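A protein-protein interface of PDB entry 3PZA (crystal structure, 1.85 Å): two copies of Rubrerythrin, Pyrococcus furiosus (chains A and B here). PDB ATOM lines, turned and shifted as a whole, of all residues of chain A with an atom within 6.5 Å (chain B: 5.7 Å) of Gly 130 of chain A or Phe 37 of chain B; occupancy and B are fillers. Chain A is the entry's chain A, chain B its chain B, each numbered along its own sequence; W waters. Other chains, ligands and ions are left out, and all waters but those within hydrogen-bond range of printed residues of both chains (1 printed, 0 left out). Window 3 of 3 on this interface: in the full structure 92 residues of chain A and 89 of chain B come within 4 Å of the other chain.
The side-chain carboxylate (OD2) of Asp 132 of chain A lies within hydrogen-bond range of the backbone NH (N) of Ile 40 of chain B (3.0 Å).
The side-chain carboxylate (OD1) of Asp 132 of chain A lies close to the backbone nitrogen (N) of Pro 38 of chain B (3.3 Å).
The backbone carbonyl oxygen (O) of Ile 133 of chain A is in hydrogen-bond range of the side-chain amide nitrogen (ND2) of Asn 39 of chain B (2.7 Å).
The side-chain carboxylate of Asp 132 of chain A is in hydrogen-bond range of the backbone NH of Asn 39 of chain B.
OG1 of Thr 68 of chain A sits at hydrogen-bond distance from OE1 of Glu 35 of chain B, 2.6 Å away.
The side-chain carboxylate of Glu 131 of chain A is in salt-bridge range of the side-chain amino group of Lys 129 of chain A, 3.99 Å away.
O of Ala 32 of chain B is in hydrogen-bond range of N of Phe 37 of chain B (2.9 Å).
The backbone carbonyl oxygen (O) of Lys 126 of chain A lies within hydrogen-bond range of the backbone NH (N) of Glu 131 of chain A (3.0 Å).
Among the printed residues, merely in contact across the chains: Thr 68 of chain A with Ala 32 of chain B, Glu 131 of chain A with Phe 37 of chain B, Asp 132 of chain A with Phe 37 of chain B, Thr 68 of chain A with Phe 37 of chain B, Thr 68 of chain A with Ile 40 of chain B, Ala 127 of chain A with Ile 40 of chain B, Ile 133 of chain A with Ile 40 of chain B and Gly 130 of chain A with Phe 37 of chain B.
Of the printed residues of chain B, Thr 68 of chain A touches Ala 32, Glu 35, Phe 37 and Ile 40.
Printed residues of chain B within 4 Å of Ala 127 of chain A: Ile 40 (3.8 Å).
Gly 130 of chain A touches just one residue of chain B: Phe 37.
The nearest printed residue of chain B that does not touch Gly 130 of chain A is Gly 36 of chain B (6.5 Å).
The nearest printed residue of chain B that does not touch Asp 132 of chain A is Gly 36 of chain B (4.6 Å).
Hydrophobic or aromatic side chains of chain A within 4 Å of the printed part of chain B: Ala 127 and Ile 133.
Of the 10 printed residues of chain B, 6 touch a printed residue of chain A.
Hydrophobic or aromatic side chains of chain B that line the printed part of chain A: Ala 32, Phe 37, Pro 38 and Ile 40.
Among the printed residues, 13 pairs touch across the chains.
Among the printed residues, no Asp or Glu carboxylate lies within 4 Å of a Lys or Arg side-chain nitrogen of the other chain.
No position is printed for both chains.
Of the 13 pairs that touch across the chains among the printed residues, none has its exchanged pair printed and touching as well.
Water W1 lies within hydrogen-bond range of the side-chain hydroxyl (OG1) of Thr 68 of chain A (2.8 Å) and the backbone NH (N) of Ala 32 of chain B (3.5 Å).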
ATOM      1  N   THR A  68       6.565 -27.299  19.521  1.00  0.00           N
ATOM      2  CA  THR A  68       6.227 -28.309  18.545  1.00  0.00           C
ATOM      3  C   THR A  68       6.757 -29.688  18.908  1.00  0.00           C
ATOM      4  O   THR A  68       5.997 -30.685  18.759  1.00  0.00           O
ATOM      5  CB  THR A  68       6.608 -27.840  17.134  1.00  0.00           C
ATOM      6  OG1 THR A  68       5.785 -26.697  16.823  1.00  0.00           O
ATOM      7  CG2 THR A  68       6.333 -28.913  16.102  1.00  0.00           C
ATOM      8  N   PRO A  69       8.053 -29.806  19.354  1.00  0.00           N
ATOM      9  CA  PRO A  69       8.446 -31.201  19.734  1.00  0.00           C
ATOM     10  C   PRO A  69       7.595 -31.820  20.843  1.00  0.00           C
ATOM     11  O   PRO A  69       7.236 -32.995  20.721  1.00  0.00           O
ATOM     12  CB  PRO A  69       9.944 -31.076  20.188  1.00  0.00           C
ATOM     13  CG  PRO A  69      10.391 -29.725  19.513  1.00  0.00           C
ATOM     14  CD  PRO A  69       9.146 -28.830  19.585  1.00  0.00           C
ATOM     15  N   GLU A 125      11.583 -36.236  15.348  1.00  0.00           N
ATOM     16  CA  GLU A 125      13.052 -36.389  15.088  1.00  0.00           C
ATOM     17  C   GLU A 125      13.601 -35.139  14.456  1.00  0.00           C
ATOM     18  O   GLU A 125      14.664 -34.658  14.840  1.00  0.00           O
ATOM     19  CB  GLU A 125      13.328 -37.583  14.155  1.00  0.00           C
ATOM     20  CG  GLU A 125      13.034 -38.972  14.778  1.00  0.00           C
ATOM     21  CD  GLU A 125      13.201 -40.147  13.762  1.00  0.00           C
ATOM     22  OE1 GLU A 125      14.294 -40.231  13.158  1.00  0.00           O
ATOM     23  OE2 GLU A 125      12.259 -40.972  13.553  1.00  0.00           O
ATOM     24  N   LYS A 126      12.910 -34.619  13.470  1.00  0.00           N
ATOM     25  CA  LYS A 126      13.331 -33.380  12.834  1.00  0.00           C
ATOM     26  C   LYS A 126      13.088 -32.158  13.678  1.00  0.00           C
ATOM     27  O   LYS A 126      14.001 -31.343  13.841  1.00  0.00           O
ATOM     28  CB  LYS A 126      12.710 -33.243  11.481  1.00  0.00           C
ATOM     29  CG  LYS A 126      13.415 -34.143  10.406  1.00  0.00           C
ATOM     30  CD  LYS A 126      12.350 -34.691   9.461  1.00  0.00           C
ATOM     31  CE  LYS A 126      12.901 -35.295   8.103  1.00  0.00           C
ATOM     32  NZ  LYS A 126      11.951 -34.981   6.918  1.00  0.00           N
ATOM     33  N   ALA A 127      11.866 -32.009  14.218  1.00  0.00           N
ATOM     34  CA  ALA A 127      11.546 -30.881  15.095  1.00  0.00           C
ATOM     35  C   ALA A 127      12.513 -30.662  16.279  1.00  0.00           C
ATOM     36  O   ALA A 127      12.951 -29.563  16.503  1.00  0.00           O
ATOM     37  CB  ALA A 127      10.040 -30.981  15.613  1.00  0.00           C
ATOM     38  N   GLU A 128      12.826 -31.716  17.035  1.00  0.00           N
ATOM     39  CA  GLU A 128      13.590 -31.588  18.257  1.00  0.00           C
ATOM     40  C   GLU A 128      15.075 -31.104  18.025  1.00  0.00           C
ATOM     41  O   GLU A 128      15.752 -30.745  18.997  1.00  0.00           O
ATOM     42  CB  GLU A 128      13.581 -32.937  19.002  1.00  0.00           C
ATOM     43  CG  GLU A 128      13.524 -32.825  20.518  1.00  0.00           C
ATOM     44  CD  GLU A 128      13.326 -34.169  21.253  1.00  0.00           C
ATOM     45  OE1 GLU A 128      13.497 -35.242  20.600  1.00  0.00           O
ATOM     46  OE2 GLU A 128      13.017 -34.148  22.492  1.00  0.00           O
ATOM     47  N   LYS A 129      15.526 -31.088  16.759  1.00  0.00           N
ATOM     48  CA  LYS A 129      16.818 -30.521  16.244  1.00  0.00           C
ATOM     49  C   LYS A 129      16.617 -29.217  15.480  1.00  0.00           C
ATOM     50  O   LYS A 129      17.426 -28.843  14.626  1.00  0.00           O
ATOM     51  CB  LYS A 129      17.427 -31.481  15.237  1.00  0.00           C
ATOM     52  CG  LYS A 129      18.186 -32.664  15.875  1.00  0.00           C
ATOM     53  CD  LYS A 129      18.377 -33.821  14.906  1.00  0.00           C
ATOM     54  CE  LYS A 129      18.301 -33.301  13.457  1.00  0.00           C
ATOM     55  NZ  LYS A 129      18.285 -34.396  12.456  1.00  0.00           N
ATOM     56  N   GLY A 130      15.474 -28.569  15.695  1.00  0.00           N
ATOM     57  CA  GLY A 130      15.166 -27.346  14.956  1.00  0.00           C
ATOM     58  C   GLY A 130      14.883 -27.391  13.477  1.00  0.00           C
ATOM     59  O   GLY A 130      14.932 -26.374  12.833  1.00  0.00           O
ATOM     60  N   GLU A 131      14.571 -28.538  12.885  1.00  0.00           N
ATOM     61  CA  GLU A 131      14.327 -28.562  11.473  1.00  0.00           C
ATOM     62  C   GLU A 131      12.850 -28.909  11.240  1.00  0.00           C
ATOM     63  O   GLU A 131      12.229 -29.609  12.048  1.00  0.00           O
ATOM     64  CB  GLU A 131      15.225 -29.611  10.816  1.00  0.00           C
ATOM     65  CG  GLU A 131      16.739 -29.432  11.249  1.00  0.00           C
ATOM     66  CD  GLU A 131      17.666 -30.562  10.755  1.00  0.00           C
ATOM     67  OE1 GLU A 131      18.831 -30.629  11.248  1.00  0.00           O
ATOM     68  OE2 GLU A 131      17.238 -31.379   9.894  1.00  0.00           O
ATOM     69  N   ASP A 132      12.334 -28.352  10.156  1.00  0.00           N
ATOM     70  CA  ASP A 132      11.018 -28.719   9.606  1.00  0.00           C
ATOM     71  C   ASP A 132      11.107 -30.039   8.843  1.00  0.00           C
ATOM     72  O   ASP A 132      12.192 -30.472   8.435  1.00  0.00           O
ATOM     73  CB  ASP A 132      10.492 -27.596   8.715  1.00  0.00           C
ATOM     74  CG  ASP A 132       9.003 -27.658   8.537  1.00  0.00           C
ATOM     75  OD1 ASP A 132       8.526 -26.852   7.744  1.00  0.00           O
ATOM     76  OD2 ASP A 132       8.310 -28.509   9.177  1.00  0.00           O
ATOM     77  N   ILE A 133      10.001 -30.731   8.686  1.00  0.00           N
ATOM     78  CA  ILE A 133      10.018 -31.926   7.873  1.00  0.00           C
ATOM     79  C   ILE A 133       9.940 -31.444   6.443  1.00  0.00           C
ATOM     80  O   ILE A 133       9.542 -30.290   6.147  1.00  0.00           O
ATOM     81  CB  ILE A 133       8.860 -32.927   8.232  1.00  0.00           C
ATOM     82  CG1 ILE A 133       7.492 -32.259   7.962  1.00  0.00           C
ATOM     83  CG2 ILE A 133       8.991 -33.314   9.677  1.00  0.00           C
ATOM     84  CD1 ILE A 133       6.345 -33.192   8.348  1.00  0.00           C
ATOM     85  N   ALA B  32       2.753 -24.703  15.383  1.00  0.00           N
ATOM     86  CA  ALA B  32       3.912 -25.080  14.540  1.00  0.00           C
ATOM     87  C   ALA B  32       4.135 -23.964  13.516  1.00  0.00           C
ATOM     88  O   ALA B  32       5.295 -23.649  13.173  1.00  0.00           O
ATOM     89  CB  ALA B  32       3.591 -26.380  13.809  1.00  0.00           C
ATOM     90  N   GLU B  33       3.067 -23.423  12.979  1.00  0.00           N
ATOM     91  CA  GLU B  33       3.112 -22.348  11.971  1.00  0.00           C
ATOM     92  C   GLU B  33       3.795 -21.132  12.640  1.00  0.00           C
ATOM     93  O   GLU B  33       4.725 -20.545  12.049  1.00  0.00           O
ATOM     94  CB  GLU B  33       1.684 -22.021  11.455  1.00  0.00           C
ATOM     95  CG  GLU B  33       1.565 -21.108  10.217  1.00  0.00           C
ATOM     96  CD  GLU B  33       1.811 -21.837   8.862  1.00  0.00           C
ATOM     97  OE1 GLU B  33       0.995 -22.692   8.428  1.00  0.00           O
ATOM     98  OE2 GLU B  33       2.832 -21.514   8.196  1.00  0.00           O
ATOM     99  N   GLU B  35       5.935 -21.131  15.178  1.00  0.00           N
ATOM    100  CA  GLU B  35       7.299 -21.470  15.489  1.00  0.00           C
ATOM    101  C   GLU B  35       8.203 -21.629  14.258  1.00  0.00           C
ATOM    102  O   GLU B  35       9.393 -21.832  14.410  1.00  0.00           O
ATOM    103  CB  GLU B  35       7.394 -22.753  16.337  1.00  0.00           C
ATOM    104  CG  GLU B  35       6.995 -22.495  17.775  1.00  0.00           C
ATOM    105  CD  GLU B  35       7.245 -23.723  18.698  1.00  0.00           C
ATOM    106  OE1 GLU B  35       6.979 -24.875  18.301  1.00  0.00           O
ATOM    107  OE2 GLU B  35       7.703 -23.538  19.841  1.00  0.00           O
ATOM    108  N   GLY B  36       7.647 -21.626  13.061  1.00  0.00           N
ATOM    109  CA  GLY B  36       8.514 -21.707  11.865  1.00  0.00           C
ATOM    110  C   GLY B  36       8.621 -23.121  11.286  1.00  0.00           C
ATOM    111  O   GLY B  36       9.601 -23.412  10.601  1.00  0.00           O
ATOM    112  N   PHE B  37       7.607 -23.977  11.526  1.00  0.00           N
ATOM    113  CA  PHE B  37       7.529 -25.308  10.952  1.00  0.00           C
ATOM    114  C   PHE B  37       6.270 -25.453  10.093  1.00  0.00           C
ATOM    115  O   PHE B  37       5.316 -26.182  10.468  1.00  0.00           O
ATOM    116  CB  PHE B  37       7.522 -26.413  12.013  1.00  0.00           C
ATOM    117  CG  PHE B  37       8.655 -26.345  13.012  1.00  0.00           C
ATOM    118  CD1 PHE B  37       8.433 -25.955  14.307  1.00  0.00           C
ATOM    119  CD2 PHE B  37       9.965 -26.731  12.649  1.00  0.00           C
ATOM    120  CE1 PHE B  37       9.489 -25.981  15.290  1.00  0.00           C
ATOM    121  CE2 PHE B  37      11.009 -26.733  13.597  1.00  0.00           C
ATOM    122  CZ  PHE B  37      10.776 -26.359  14.917  1.00  0.00           C
ATOM    123  N   PRO B  38       6.269 -24.818   8.920  1.00  0.00           N
ATOM    124  CA  PRO B  38       5.049 -24.848   8.120  1.00  0.00           C
ATOM    125  C   PRO B  38       4.682 -26.277   7.575  1.00  0.00           C
ATOM    126  O   PRO B  38       3.512 -26.548   7.326  1.00  0.00           O
ATOM    127  CB  PRO B  38       5.326 -23.857   6.992  1.00  0.00           C
ATOM    128  CG  PRO B  38       6.866 -23.911   6.790  1.00  0.00           C
ATOM    129  CD  PRO B  38       7.404 -24.132   8.248  1.00  0.00           C
ATOM    130  N   ASN B  39       5.668 -27.172   7.377  1.00  0.00           N
ATOM    131  CA  ASN B  39       5.346 -28.515   6.849  1.00  0.00           C
ATOM    132  C   ASN B  39       4.799 -29.372   7.976  1.00  0.00           C
ATOM    133  O   ASN B  39       3.869 -30.132   7.690  1.00  0.00           O
ATOM    134  CB  ASN B  39       6.545 -29.190   6.172  1.00  0.00           C
ATOM    135  CG  ASN B  39       6.913 -28.501   4.888  1.00  0.00           C
ATOM    136  OD1 ASN B  39       6.047 -27.919   4.217  1.00  0.00           O
ATOM    137  ND2 ASN B  39       8.175 -28.634   4.482  1.00  0.00           N
ATOM    138  N   ILE B  40       5.391 -29.272   9.173  1.00  0.00           N
ATOM    139  CA  ILE B  40       4.796 -29.854  10.387  1.00  0.00           C
ATOM    140  C   ILE B  40       3.334 -29.349  10.605  1.00  0.00           C
ATOM    141  O   ILE B  40       2.448 -30.159  10.951  1.00  0.00           O
ATOM    142  CB  ILE B  40       5.661 -29.669  11.610  1.00  0.00           C
ATOM    143  CG1 ILE B  40       6.919 -30.566  11.446  1.00  0.00           C
ATOM    144  CG2 ILE B  40       4.948 -30.221  12.841  1.00  0.00           C
ATOM    145  CD1 ILE B  40       7.797 -30.489  12.558  1.00  0.00           C
ATOM    146  N   ALA B  41       3.094 -28.054  10.382  1.00  0.00           N
ATOM    147  CA  ALA B  41       1.690 -27.534  10.480  1.00  0.00           C
ATOM    148  C   ALA B  41       0.774 -28.211   9.474  1.00  0.00           C
ATOM    149  O   ALA B  41      -0.369 -28.600   9.801  1.00  0.00           O
ATOM    150  CB  ALA B  41       1.694 -26.012  10.271  1.00  0.00           C
ATOM    151  N   LYS B  42       1.266 -28.388   8.223  1.00  0.00           N
ATOM    152  CA  LYS B  42       0.489 -28.987   7.171  1.00  0.00           C
ATOM    153  C   LYS B  42       0.141 -30.431   7.567  1.00  0.00           C
ATOM    154  O   LYS B  42      -1.051 -30.874   7.378  1.00  0.00           O
ATOM    155  CB  LYS B  42       1.326 -28.922   5.850  1.00  0.00           C
ATOM    156  CG  LYS B  42       0.571 -29.535   4.657  1.00  0.00           C
ATOM    157  CD  LYS B  42       1.533 -29.917   3.466  1.00  0.00           C
ATOM    158  CE  LYS B  42       2.710 -28.988   3.267  1.00  0.00           C
ATOM    159  NZ  LYS B  42       2.297 -27.701   2.678  1.00  0.00           N
HETATM  160  O   HOH W   1       3.112 -27.532  17.332  1.00  0.00           O
